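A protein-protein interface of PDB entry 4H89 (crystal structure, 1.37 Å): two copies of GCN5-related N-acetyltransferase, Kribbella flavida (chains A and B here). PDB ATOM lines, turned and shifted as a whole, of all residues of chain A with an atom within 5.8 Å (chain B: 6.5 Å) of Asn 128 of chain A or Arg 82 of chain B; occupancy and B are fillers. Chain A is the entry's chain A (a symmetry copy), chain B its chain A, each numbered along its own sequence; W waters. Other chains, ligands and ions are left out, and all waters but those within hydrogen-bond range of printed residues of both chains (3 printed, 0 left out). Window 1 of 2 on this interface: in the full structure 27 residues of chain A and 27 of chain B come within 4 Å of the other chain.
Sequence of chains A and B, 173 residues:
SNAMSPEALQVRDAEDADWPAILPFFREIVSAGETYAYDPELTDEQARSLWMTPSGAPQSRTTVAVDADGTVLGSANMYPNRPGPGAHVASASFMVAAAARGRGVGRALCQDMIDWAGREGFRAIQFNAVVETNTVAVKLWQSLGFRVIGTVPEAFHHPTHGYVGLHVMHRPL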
ATOM      1  N   ALA A  37     -11.697 -11.123   7.814  1.00  0.00           N
ATOM      2  CA  ALA A  37     -11.094 -10.973   6.490  1.00  0.00           C
ATOM      3  C   ALA A  37     -10.173  -9.743   6.443  1.00  0.00           C
ATOM      4  O   ALA A  37     -10.643  -8.612   6.458  1.00  0.00           O
ATOM      5  CB  ALA A  37     -12.184 -10.854   5.428  1.00  0.00           C
ATOM      6  N   ASN A  81     -19.103   3.459  13.148  1.00  0.00           N
ATOM      7  CA  ASN A  81     -19.167   2.486  12.076  1.00  0.00           C
ATOM      8  C   ASN A  81     -19.151   3.118  10.716  1.00  0.00           C
ATOM      9  O   ASN A  81     -18.657   2.524   9.779  1.00  0.00           O
ATOM     10  CB  ASN A  81     -20.385   1.581  12.195  1.00  0.00           C
ATOM     11  CG  ASN A  81     -20.223   0.277  11.406  1.00  0.00           C
ATOM     12  OD1 ASN A  81     -19.128  -0.316  11.377  1.00  0.00           O
ATOM     13  ND2 ASN A  81     -21.284  -0.172  10.772  1.00  0.00           N
ATOM     14  N   ARG A  82     -19.754   4.299  10.607  1.00  0.00           N
ATOM     15  CA  ARG A  82     -19.842   5.058   9.384  1.00  0.00           C
ATOM     16  C   ARG A  82     -19.719   6.529   9.777  1.00  0.00           C
ATOM     17  O   ARG A  82     -20.011   6.900  10.879  1.00  0.00           O
ATOM     18  CB  ARG A  82     -21.220   4.840   8.681  1.00  0.00           C
ATOM     19  CG  ARG A  82     -21.353   3.414   8.184  1.00  0.00           C
ATOM     20  CD  ARG A  82     -22.671   3.038   7.515  1.00  0.00           C
ATOM     21  NE  ARG A  82     -22.364   1.906   6.609  1.00  0.00           N
ATOM     22  CZ  ARG A  82     -22.576   0.620   6.868  1.00  0.00           C
ATOM     23  NH1 ARG A  82     -22.140  -0.283   5.994  1.00  0.00           N
ATOM     24  NH2 ARG A  82     -23.280   0.217   7.939  1.00  0.00           N
ATOM     25  N   SER A  91     -18.844   0.756  16.138  1.00  0.00           N
ATOM     26  CA  SER A  91     -18.439  -0.633  15.888  1.00  0.00           C
ATOM     27  C   SER A  91     -17.148  -0.880  16.602  1.00  0.00           C
ATOM     28  O   SER A  91     -16.578   0.012  17.238  1.00  0.00           O
ATOM     29  CB  SER A  91     -18.297  -0.836  14.397  1.00  0.00           C
ATOM     30  OG  SER A  91     -18.071  -2.220  14.070  1.00  0.00           O
ATOM     31  N   GLN A 126     -22.821  -1.880  15.945  1.00  0.00           N
ATOM     32  CA  GLN A 126     -23.001  -2.816  14.845  1.00  0.00           C
ATOM     33  C   GLN A 126     -21.680  -3.529  14.589  1.00  0.00           C
ATOM     34  O   GLN A 126     -20.627  -2.883  14.540  1.00  0.00           O
ATOM     35  CB  GLN A 126     -23.415  -2.028  13.595  1.00  0.00           C
ATOM     36  CG  GLN A 126     -23.591  -2.828  12.336  1.00  0.00           C
ATOM     37  CD  GLN A 126     -24.148  -2.019  11.219  1.00  0.00           C
ATOM     38  OE1 GLN A 126     -24.895  -1.028  11.431  1.00  0.00           O
ATOM     39  NE2 GLN A 126     -23.845  -2.434  10.009  1.00  0.00           N
ATOM     40  N   PHE A 127     -21.746  -4.850  14.390  1.00  0.00           N
ATOM     41  CA  PHE A 127     -20.612  -5.638  13.870  1.00  0.00           C
ATOM     42  C   PHE A 127     -21.002  -6.038  12.447  1.00  0.00           C
ATOM     43  O   PHE A 127     -22.001  -6.716  12.248  1.00  0.00           O
ATOM     44  CB  PHE A 127     -20.345  -6.895  14.737  1.00  0.00           C
ATOM     45  CG  PHE A 127     -19.980  -6.601  16.152  1.00  0.00           C
ATOM     46  CD1 PHE A 127     -19.445  -5.362  16.566  1.00  0.00           C
ATOM     47  CD2 PHE A 127     -20.225  -7.543  17.125  1.00  0.00           C
ATOM     48  CE1 PHE A 127     -19.073  -5.142  17.897  1.00  0.00           C
ATOM     49  CE2 PHE A 127     -19.856  -7.366  18.437  1.00  0.00           C
ATOM     50  CZ  PHE A 127     -19.299  -6.147  18.845  1.00  0.00           C
ATOM     51  N   ASN A 128     -20.202  -5.618  11.467  1.00  0.00           N
ATOM     52  CA  ASN A 128     -20.575  -5.783  10.088  1.00  0.00           C
ATOM     53  C   ASN A 128     -20.456  -7.193   9.561  1.00  0.00           C
ATOM     54  O   ASN A 128     -21.138  -7.544   8.600  1.00  0.00           O
ATOM     55  CB  ASN A 128     -19.724  -4.847   9.242  1.00  0.00           C
ATOM     56  CG  ASN A 128     -19.862  -3.452   9.720  1.00  0.00           C
ATOM     57  OD1 ASN A 128     -20.991  -2.926   9.711  1.00  0.00           O
ATOM     58  ND2 ASN A 128     -18.770  -2.894  10.321  1.00  0.00           N
ATOM     59  N   ALA A 129     -19.557  -7.976  10.159  1.00  0.00           N
ATOM     60  CA  ALA A 129     -19.220  -9.275   9.624  1.00  0.00           C
ATOM     61  C   ALA A 129     -18.687 -10.176  10.705  1.00  0.00           C
ATOM     62  O   ALA A 129     -17.557 -10.042  11.171  1.00  0.00           O
ATOM     63  CB  ALA A 129     -18.184  -9.129   8.537  1.00  0.00           C
ATOM     64  N   VAL A 130     -19.517 -11.069  11.183  1.00  0.00           N
ATOM     65  CA  VAL A 130     -19.165 -12.046  12.165  1.00  0.00           C
ATOM     66  C   VAL A 130     -19.305 -13.425  11.512  1.00  0.00           C
ATOM     67  O   VAL A 130     -20.340 -13.770  10.991  1.00  0.00           O
ATOM     68  CB  VAL A 130     -20.031 -11.985  13.435  1.00  0.00           C
ATOM     69  CG1 VAL A 130     -19.505 -12.999  14.432  1.00  0.00           C
ATOM     70  CG2 VAL A 130     -20.041 -10.557  14.001  1.00  0.00           C
ATOM     71  N   ALA A 155     -20.326 -15.868   2.308  1.00  0.00           N
ATOM     72  CA  ALA A 155     -19.545 -14.642   2.136  1.00  0.00           C
ATOM     73  C   ALA A 155     -18.105 -14.730   2.639  1.00  0.00           C
ATOM     74  O   ALA A 155     -17.335 -13.784   2.528  1.00  0.00           O
ATOM     75  CB  ALA A 155     -20.248 -13.455   2.766  1.00  0.00           C
ATOM     76  N   LEU A 166     -21.611 -14.595   6.747  1.00  0.00           N
ATOM     77  CA  LEU A 166     -21.194 -13.501   7.593  1.00  0.00           C
ATOM     78  C   LEU A 166     -22.437 -12.831   8.210  1.00  0.00           C
ATOM     79  O   LEU A 166     -23.244 -12.270   7.476  1.00  0.00           O
ATOM     80  CB  LEU A 166     -20.379 -12.481   6.789  1.00  0.00           C
ATOM     81  CG  LEU A 166     -18.971 -12.897   6.341  1.00  0.00           C
ATOM     82  CD1 LEU A 166     -18.372 -11.773   5.506  1.00  0.00           C
ATOM     83  CD2 LEU A 166     -18.076 -13.234   7.550  1.00  0.00           C
ATOM     84  N   HIS A 167     -22.578 -12.905   9.532  1.00  0.00           N
ATOM     85  CA  HIS A 167     -23.669 -12.261  10.215  1.00  0.00           C
ATOM     86  C   HIS A 167     -23.391 -10.763  10.280  1.00  0.00           C
ATOM     87  O   HIS A 167     -22.241 -10.353  10.504  1.00  0.00           O
ATOM     88  CB  HIS A 167     -23.757 -12.713  11.654  1.00  0.00           C
ATOM     89  CG  HIS A 167     -24.050 -14.140  11.894  1.00  0.00           C
ATOM     90  ND1 HIS A 167     -25.038 -14.878  11.303  1.00  0.00           N
ATOM     91  CD2 HIS A 167     -23.454 -14.942  12.800  1.00  0.00           C
ATOM     92  CE1 HIS A 167     -25.023 -16.093  11.841  1.00  0.00           C
ATOM     93  NE2 HIS A 167     -24.065 -16.147  12.744  1.00  0.00           N
ATOM     94  N   VAL A 168     -24.462  -9.976  10.217  1.00  0.00           N
ATOM     95  CA  VAL A 168     -24.431  -8.596  10.663  1.00  0.00           C
ATOM     96  C   VAL A 168     -25.109  -8.606  12.024  1.00  0.00           C
ATOM     97  O   VAL A 168     -26.196  -9.145  12.140  1.00  0.00           O
ATOM     98  CB  VAL A 168     -25.223  -7.701   9.686  1.00  0.00           C
ATOM     99  CG1 VAL A 168     -25.237  -6.251  10.200  1.00  0.00           C
ATOM    100  CG2 VAL A 168     -24.586  -7.813   8.297  1.00  0.00           C
ATOM    101  N   MET A 169     -24.460  -8.067  13.047  1.00  0.00           N
ATOM    102  CA  MET A 169     -24.975  -8.094  14.398  1.00  0.00           C
ATOM    103  C   MET A 169     -25.137  -6.671  14.918  1.00  0.00           C
ATOM    104  O   MET A 169     -24.429  -5.759  14.503  1.00  0.00           O
ATOM    105  CB  MET A 169     -24.107  -8.867  15.346  1.00  0.00           C
ATOM    106  CG  MET A 169     -23.906 -10.302  14.851  1.00  0.00           C
ATOM    107  SD  MET A 169     -23.088 -11.536  16.103  1.00  0.00           S
ATOM    108  CE  MET A 169     -24.499 -11.861  17.389  1.00  0.00           C
ATOM    109  N   TYR B  79     -15.536  -3.374  -6.728  1.00  0.00           N
ATOM    110  CA  TYR B  79     -14.317  -3.815  -6.039  1.00  0.00           C
ATOM    111  C   TYR B  79     -14.695  -5.022  -5.169  1.00  0.00           C
ATOM    112  O   TYR B  79     -15.861  -5.217  -4.895  1.00  0.00           O
ATOM    113  CB  TYR B  79     -13.771  -2.650  -5.132  1.00  0.00           C
ATOM    114  CG  TYR B  79     -14.885  -1.903  -4.428  1.00  0.00           C
ATOM    115  CD1 TYR B  79     -15.453  -2.348  -3.241  1.00  0.00           C
ATOM    116  CD2 TYR B  79     -15.400  -0.762  -4.983  1.00  0.00           C
ATOM    117  CE1 TYR B  79     -16.547  -1.682  -2.649  1.00  0.00           C
ATOM    118  CE2 TYR B  79     -16.460  -0.083  -4.414  1.00  0.00           C
ATOM    119  CZ  TYR B  79     -17.037  -0.529  -3.265  1.00  0.00           C
ATOM    120  OH  TYR B  79     -18.106   0.187  -2.753  1.00  0.00           O
ATOM    121  N   PRO B  80     -13.723  -5.751  -4.643  1.00  0.00           N
ATOM    122  CA  PRO B  80     -14.073  -6.784  -3.668  1.00  0.00           C
ATOM    123  C   PRO B  80     -14.618  -6.152  -2.385  1.00  0.00           C
ATOM    124  O   PRO B  80     -14.061  -5.141  -1.885  1.00  0.00           O
ATOM    125  CB  PRO B  80     -12.737  -7.527  -3.420  1.00  0.00           C
ATOM    126  CG  PRO B  80     -11.871  -7.139  -4.599  1.00  0.00           C
ATOM    127  CD  PRO B  80     -12.291  -5.746  -4.929  1.00  0.00           C
ATOM    128  N   ASN B  81     -15.667  -6.713  -1.807  1.00  0.00           N
ATOM    129  CA  ASN B  81     -16.262  -6.129  -0.622  1.00  0.00           C
ATOM    130  C   ASN B  81     -15.375  -6.228   0.583  1.00  0.00           C
ATOM    131  O   ASN B  81     -15.428  -5.374   1.444  1.00  0.00           O
ATOM    132  CB  ASN B  81     -17.618  -6.742  -0.299  1.00  0.00           C
ATOM    133  CG  ASN B  81     -18.466  -5.842   0.607  1.00  0.00           C
ATOM    134  OD1 ASN B  81     -18.471  -4.607   0.449  1.00  0.00           O
ATOM    135  ND2 ASN B  81     -19.172  -6.436   1.545  1.00  0.00           N
ATOM    136  N   ARG B  82     -14.610  -7.313   0.664  1.00  0.00           N
ATOM    137  CA  ARG B  82     -13.694  -7.584   1.745  1.00  0.00           C
ATOM    138  C   ARG B  82     -12.476  -8.264   1.122  1.00  0.00           C
ATOM    139  O   ARG B  82     -12.565  -8.859   0.086  1.00  0.00           O
ATOM    140  CB  ARG B  82     -14.329  -8.553   2.794  1.00  0.00           C
ATOM    141  CG  ARG B  82     -15.487  -7.889   3.513  1.00  0.00           C
ATOM    142  CD  ARG B  82     -16.238  -8.734   4.536  1.00  0.00           C
ATOM    143  NE  ARG B  82     -16.843  -7.778   5.493  1.00  0.00           N
ATOM    144  CZ  ARG B  82     -18.105  -7.361   5.487  1.00  0.00           C
ATOM    145  NH1 ARG B  82     -18.463  -6.412   6.347  1.00  0.00           N
ATOM    146  NH2 ARG B  82     -19.035  -7.922   4.696  1.00  0.00           N
ATOM    147  N   PRO B  83     -11.336  -8.145   1.781  1.00  0.00           N
ATOM    148  CA  PRO B  83     -10.125  -8.760   1.244  1.00  0.00           C
ATOM    149  C   PRO B  83     -10.018 -10.216   1.628  1.00  0.00           C
ATOM    150  O   PRO B  83     -10.824 -10.759   2.376  1.00  0.00           O
ATOM    151  CB  PRO B  83      -9.013  -7.947   1.914  1.00  0.00           C
ATOM    152  CG  PRO B  83      -9.603  -7.568   3.224  1.00  0.00           C
ATOM    153  CD  PRO B  83     -11.073  -7.307   2.945  1.00  0.00           C
ATOM    154  N   GLY B  84      -8.981 -10.852   1.116  1.00  0.00           N
ATOM    155  CA  GLY B  84      -8.653 -12.208   1.511  1.00  0.00           C
ATOM    156  C   GLY B  84      -9.803 -13.186   1.367  1.00  0.00           C
ATOM    157  O   GLY B  84     -10.366 -13.370   0.295  1.00  0.00           O
ATOM    158  N   PRO B  85     -10.193 -13.822   2.494  1.00  0.00           N
ATOM    159  CA  PRO B  85     -11.220 -14.846   2.397  1.00  0.00           C
ATOM    160  C   PRO B  85     -12.625 -14.321   2.173  1.00  0.00           C
ATOM    161  O   PRO B  85     -13.541 -15.110   2.044  1.00  0.00           O
ATOM    162  CB  PRO B  85     -11.102 -15.574   3.736  1.00  0.00           C
ATOM    163  CG  PRO B  85     -10.623 -14.530   4.678  1.00  0.00           C
ATOM    164  CD  PRO B  85      -9.676 -13.701   3.858  1.00  0.00           C
ATOM    165  N   GLY B  86     -12.776 -13.003   2.063  1.00  0.00           N
ATOM    166  CA  GLY B  86     -14.061 -12.452   1.628  1.00  0.00           C
ATOM    167  C   GLY B  86     -14.089 -11.863   0.230  1.00  0.00           C
ATOM    168  O   GLY B  86     -15.115 -11.294  -0.174  1.00  0.00           O
ATOM    169  N   ALA B  87     -12.989 -11.996  -0.512  1.00  0.00           N
ATOM    170  CA  ALA B  87     -12.812 -11.269  -1.737  1.00  0.00           C
ATOM    171  C   ALA B  87     -13.666 -11.782  -2.926  1.00  0.00           C
ATOM    172  O   ALA B  87     -13.671 -11.192  -3.999  1.00  0.00           O
ATOM    173  CB  ALA B  87     -11.365 -11.231  -2.110  1.00  0.00           C
ATOM    174  N   HIS B  88     -14.321 -12.930  -2.754  1.00  0.00           N
ATOM    175  CA  HIS B  88     -15.189 -13.475  -3.772  1.00  0.00           C
ATOM    176  C   HIS B  88     -16.575 -12.815  -3.825  1.00  0.00           C
ATOM    177  O   HIS B  88     -17.379 -13.138  -4.695  1.00  0.00           O
ATOM    178  CB  HIS B  88     -15.362 -14.990  -3.558  1.00  0.00           C
ATOM    179  CG  HIS B  88     -15.912 -15.326  -2.232  1.00  0.00           C
ATOM    180  ND1 HIS B  88     -15.162 -15.236  -1.082  1.00  0.00           N
ATOM    181  CD2 HIS B  88     -17.165 -15.640  -1.856  1.00  0.00           C
ATOM    182  CE1 HIS B  88     -15.923 -15.523  -0.044  1.00  0.00           C
ATOM    183  NE2 HIS B  88     -17.149 -15.772  -0.498  1.00  0.00           N
ATOM    184  N   VAL B  89     -16.803 -11.869  -2.908  1.00  0.00           N
ATOM    185  CA  VAL B  89     -18.021 -11.091  -2.918  1.00  0.00           C
ATOM    186  C   VAL B  89     -17.633  -9.667  -3.365  1.00  0.00           C
ATOM    187  O   VAL B  89     -16.793  -9.042  -2.725  1.00  0.00           O
ATOM    188  CB  VAL B  89     -18.672 -11.037  -1.530  1.00  0.00           C
ATOM    189  CG1 VAL B  89     -19.960 -10.241  -1.578  1.00  0.00           C
ATOM    190  CG2 VAL B  89     -18.949 -12.424  -0.985  1.00  0.00           C
ATOM    191  N   GLN B 126     -22.618  -7.668  -2.774  1.00  0.00           N
ATOM    192  CA  GLN B 126     -23.227  -7.197  -1.539  1.00  0.00           C
ATOM    193  C   GLN B 126     -23.177  -5.675  -1.518  1.00  0.00           C
ATOM    194  O   GLN B 126     -22.135  -5.086  -1.828  1.00  0.00           O
ATOM    195  CB  GLN B 126     -22.428  -7.758  -0.355  1.00  0.00           C
ATOM    196  CG  GLN B 126     -22.879  -7.328   1.011  1.00  0.00           C
ATOM    197  CD  GLN B 126     -22.160  -8.041   2.101  1.00  0.00           C
ATOM    198  OE1 GLN B 126     -21.701  -9.202   1.939  1.00  0.00           O
ATOM    199  NE2 GLN B 126     -22.077  -7.398   3.245  1.00  0.00           N
ATOM    200  N   ASN B 128     -23.521  -2.917   1.409  1.00  0.00           N
ATOM    201  CA  ASN B 128     -23.487  -2.953   2.847  1.00  0.00           C
ATOM    202  C   ASN B 128     -24.509  -2.076   3.529  1.00  0.00           C
ATOM    203  O   ASN B 128     -24.879  -2.344   4.671  1.00  0.00           O
ATOM    204  CB  ASN B 128     -22.090  -2.562   3.307  1.00  0.00           C
ATOM    205  CG  ASN B 128     -21.076  -3.441   2.679  1.00  0.00           C
ATOM    206  OD1 ASN B 128     -21.134  -4.666   2.892  1.00  0.00           O
ATOM    207  ND2 ASN B 128     -20.254  -2.870   1.750  1.00  0.00           N
HETATM  208  O   HOH W   1     -17.117 -11.129   1.757  1.00  0.00           O
HETATM  209  O   HOH W   2     -21.963  -5.760   6.201  1.00  0.00           O
HETATM  210  O   HOH W   3     -23.127  -3.581   6.911  1.00  0.00           O
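The side-chain amide oxygen (OD1) of Asn 81 of chain B is in hydrogen-bond range of the side-chain amide nitrogen (ND2) of Asn 128 of chain B (2.8 Å). The backbone NH of Asn 81 of chain B lies within hydrogen-bond range of the backbone carbonyl oxygen of Val 89 of chain B. ND2 of Asn 81 of chain B sits close to NH2 of Arg 82 of chain B, 3.5 Å away. NE2 of Gln 126 of chain A sits close to NH2 of Arg 82 of chain A (3.4 Å). The backbone carbonyl oxygen of Arg 82 of chain B sits close to the backbone NH of Ala 87 of chain B, at 3.2 Å. NE2 of Gln 126 of chain B lies within hydrogen-bond range of OD1 of Asn 128 of chain B (2.9 Å).
O of Pro 83 of chain B touches CB of Ala 37 of chain A, at 3.3 Å. Arg 82 of chain A touches Asn 128 of chain B (NH1 to CB, 3.5 Å). NH1 of Arg 82 of chain B touches CB of Asn 128 of chain A, at 3.5 Å. Ala 129 of chain A touches Arg 82 of chain B. O of Ala 155 of chain A touches CA of Gly 86 of chain B, at 3.6 Å. O of Ala 155 of chain A touches CE1 of His 88 of chain B, at 3.4 Å. Val 89 of chain B touches Ala 155 of chain A. CD1 of Leu 166 of chain A touches CD of Arg 82 of chain B, at 3.8 Å.
Water W1 bridges the backbone carbonyl oxygen (O) of Ala 155 of chain A (2.8 Å) and the backbone carbonyl oxygen (O) of Gly 86 of chain B (2.8 Å). Water W3 bridges the backbone carbonyl oxygen (O) of Asn 128 of chain B (3.1 Å) and the side-chain amide nitrogen (NE2) of Gln 126 of chain A (3.4 Å). Water W2 lies within hydrogen-bond range of the backbone carbonyl oxygen (O) of Asn 128 of chain A (3.1 Å) and the side-chain amide nitrogen (NE2) of Gln 126 of chain B (3.4 Å).
Of chain B, only Arg 82 comes within 4 Å of Asn 128 of chain A. Of chain A, only Asn 128, Ala 129 and Leu 166 come within 4 Å of Arg 82 of chain B. Printed residues of chain A within 4 Å of Asn 128 of chain B: Arg 82 (3.5 Å). Printed residues of chain B within 4 Å of Ala 155 of chain A: Gly 86 (3.6 Å), His 88 (3.4 Å) and Val 89 (3.9 Å). Of the printed residues of chain B, Arg 82 of chain A touches Asn 128. Of the printed residues of chain A, Pro 83 of chain B touches Ala 37 (3.3 Å). Met 169 of chain A touches none of the printed residues of chain B. Val 130 of chain A touches none of the printed residues of chain B. The nearest residue of chain A that does not touch Arg 82 of chain B is Ala 37 of chain A (4.1 Å). The nearest printed residue of chain A that does not touch Val 89 of chain B is Leu 166 of chain A (6.5 Å).
Printed residues of chain A that touch a printed residue of chain B: Ala 37, Arg 82, Asn 128, Ala 129, Ala 155 and Leu 166. Printed residues of chain B that touch a printed residue of chain A: Arg 82, Pro 83, Gly 86, His 88, Val 89 and Asn 128. Hydrophobic or aromatic side chains of chain B that line the printed part of chain A: Pro 83, His 88 and Val 89. Among the printed residues, 8 pairs touch across the chains.
Arg 82 of chain A touches Asn 128 of chain B, and with the chains exchanged Asn 128 of chain A touches Arg 82 of chain B. Of the 8 pairs that touch across the chains among the printed residues, 2 have their exchanged pair printed and touching as well.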
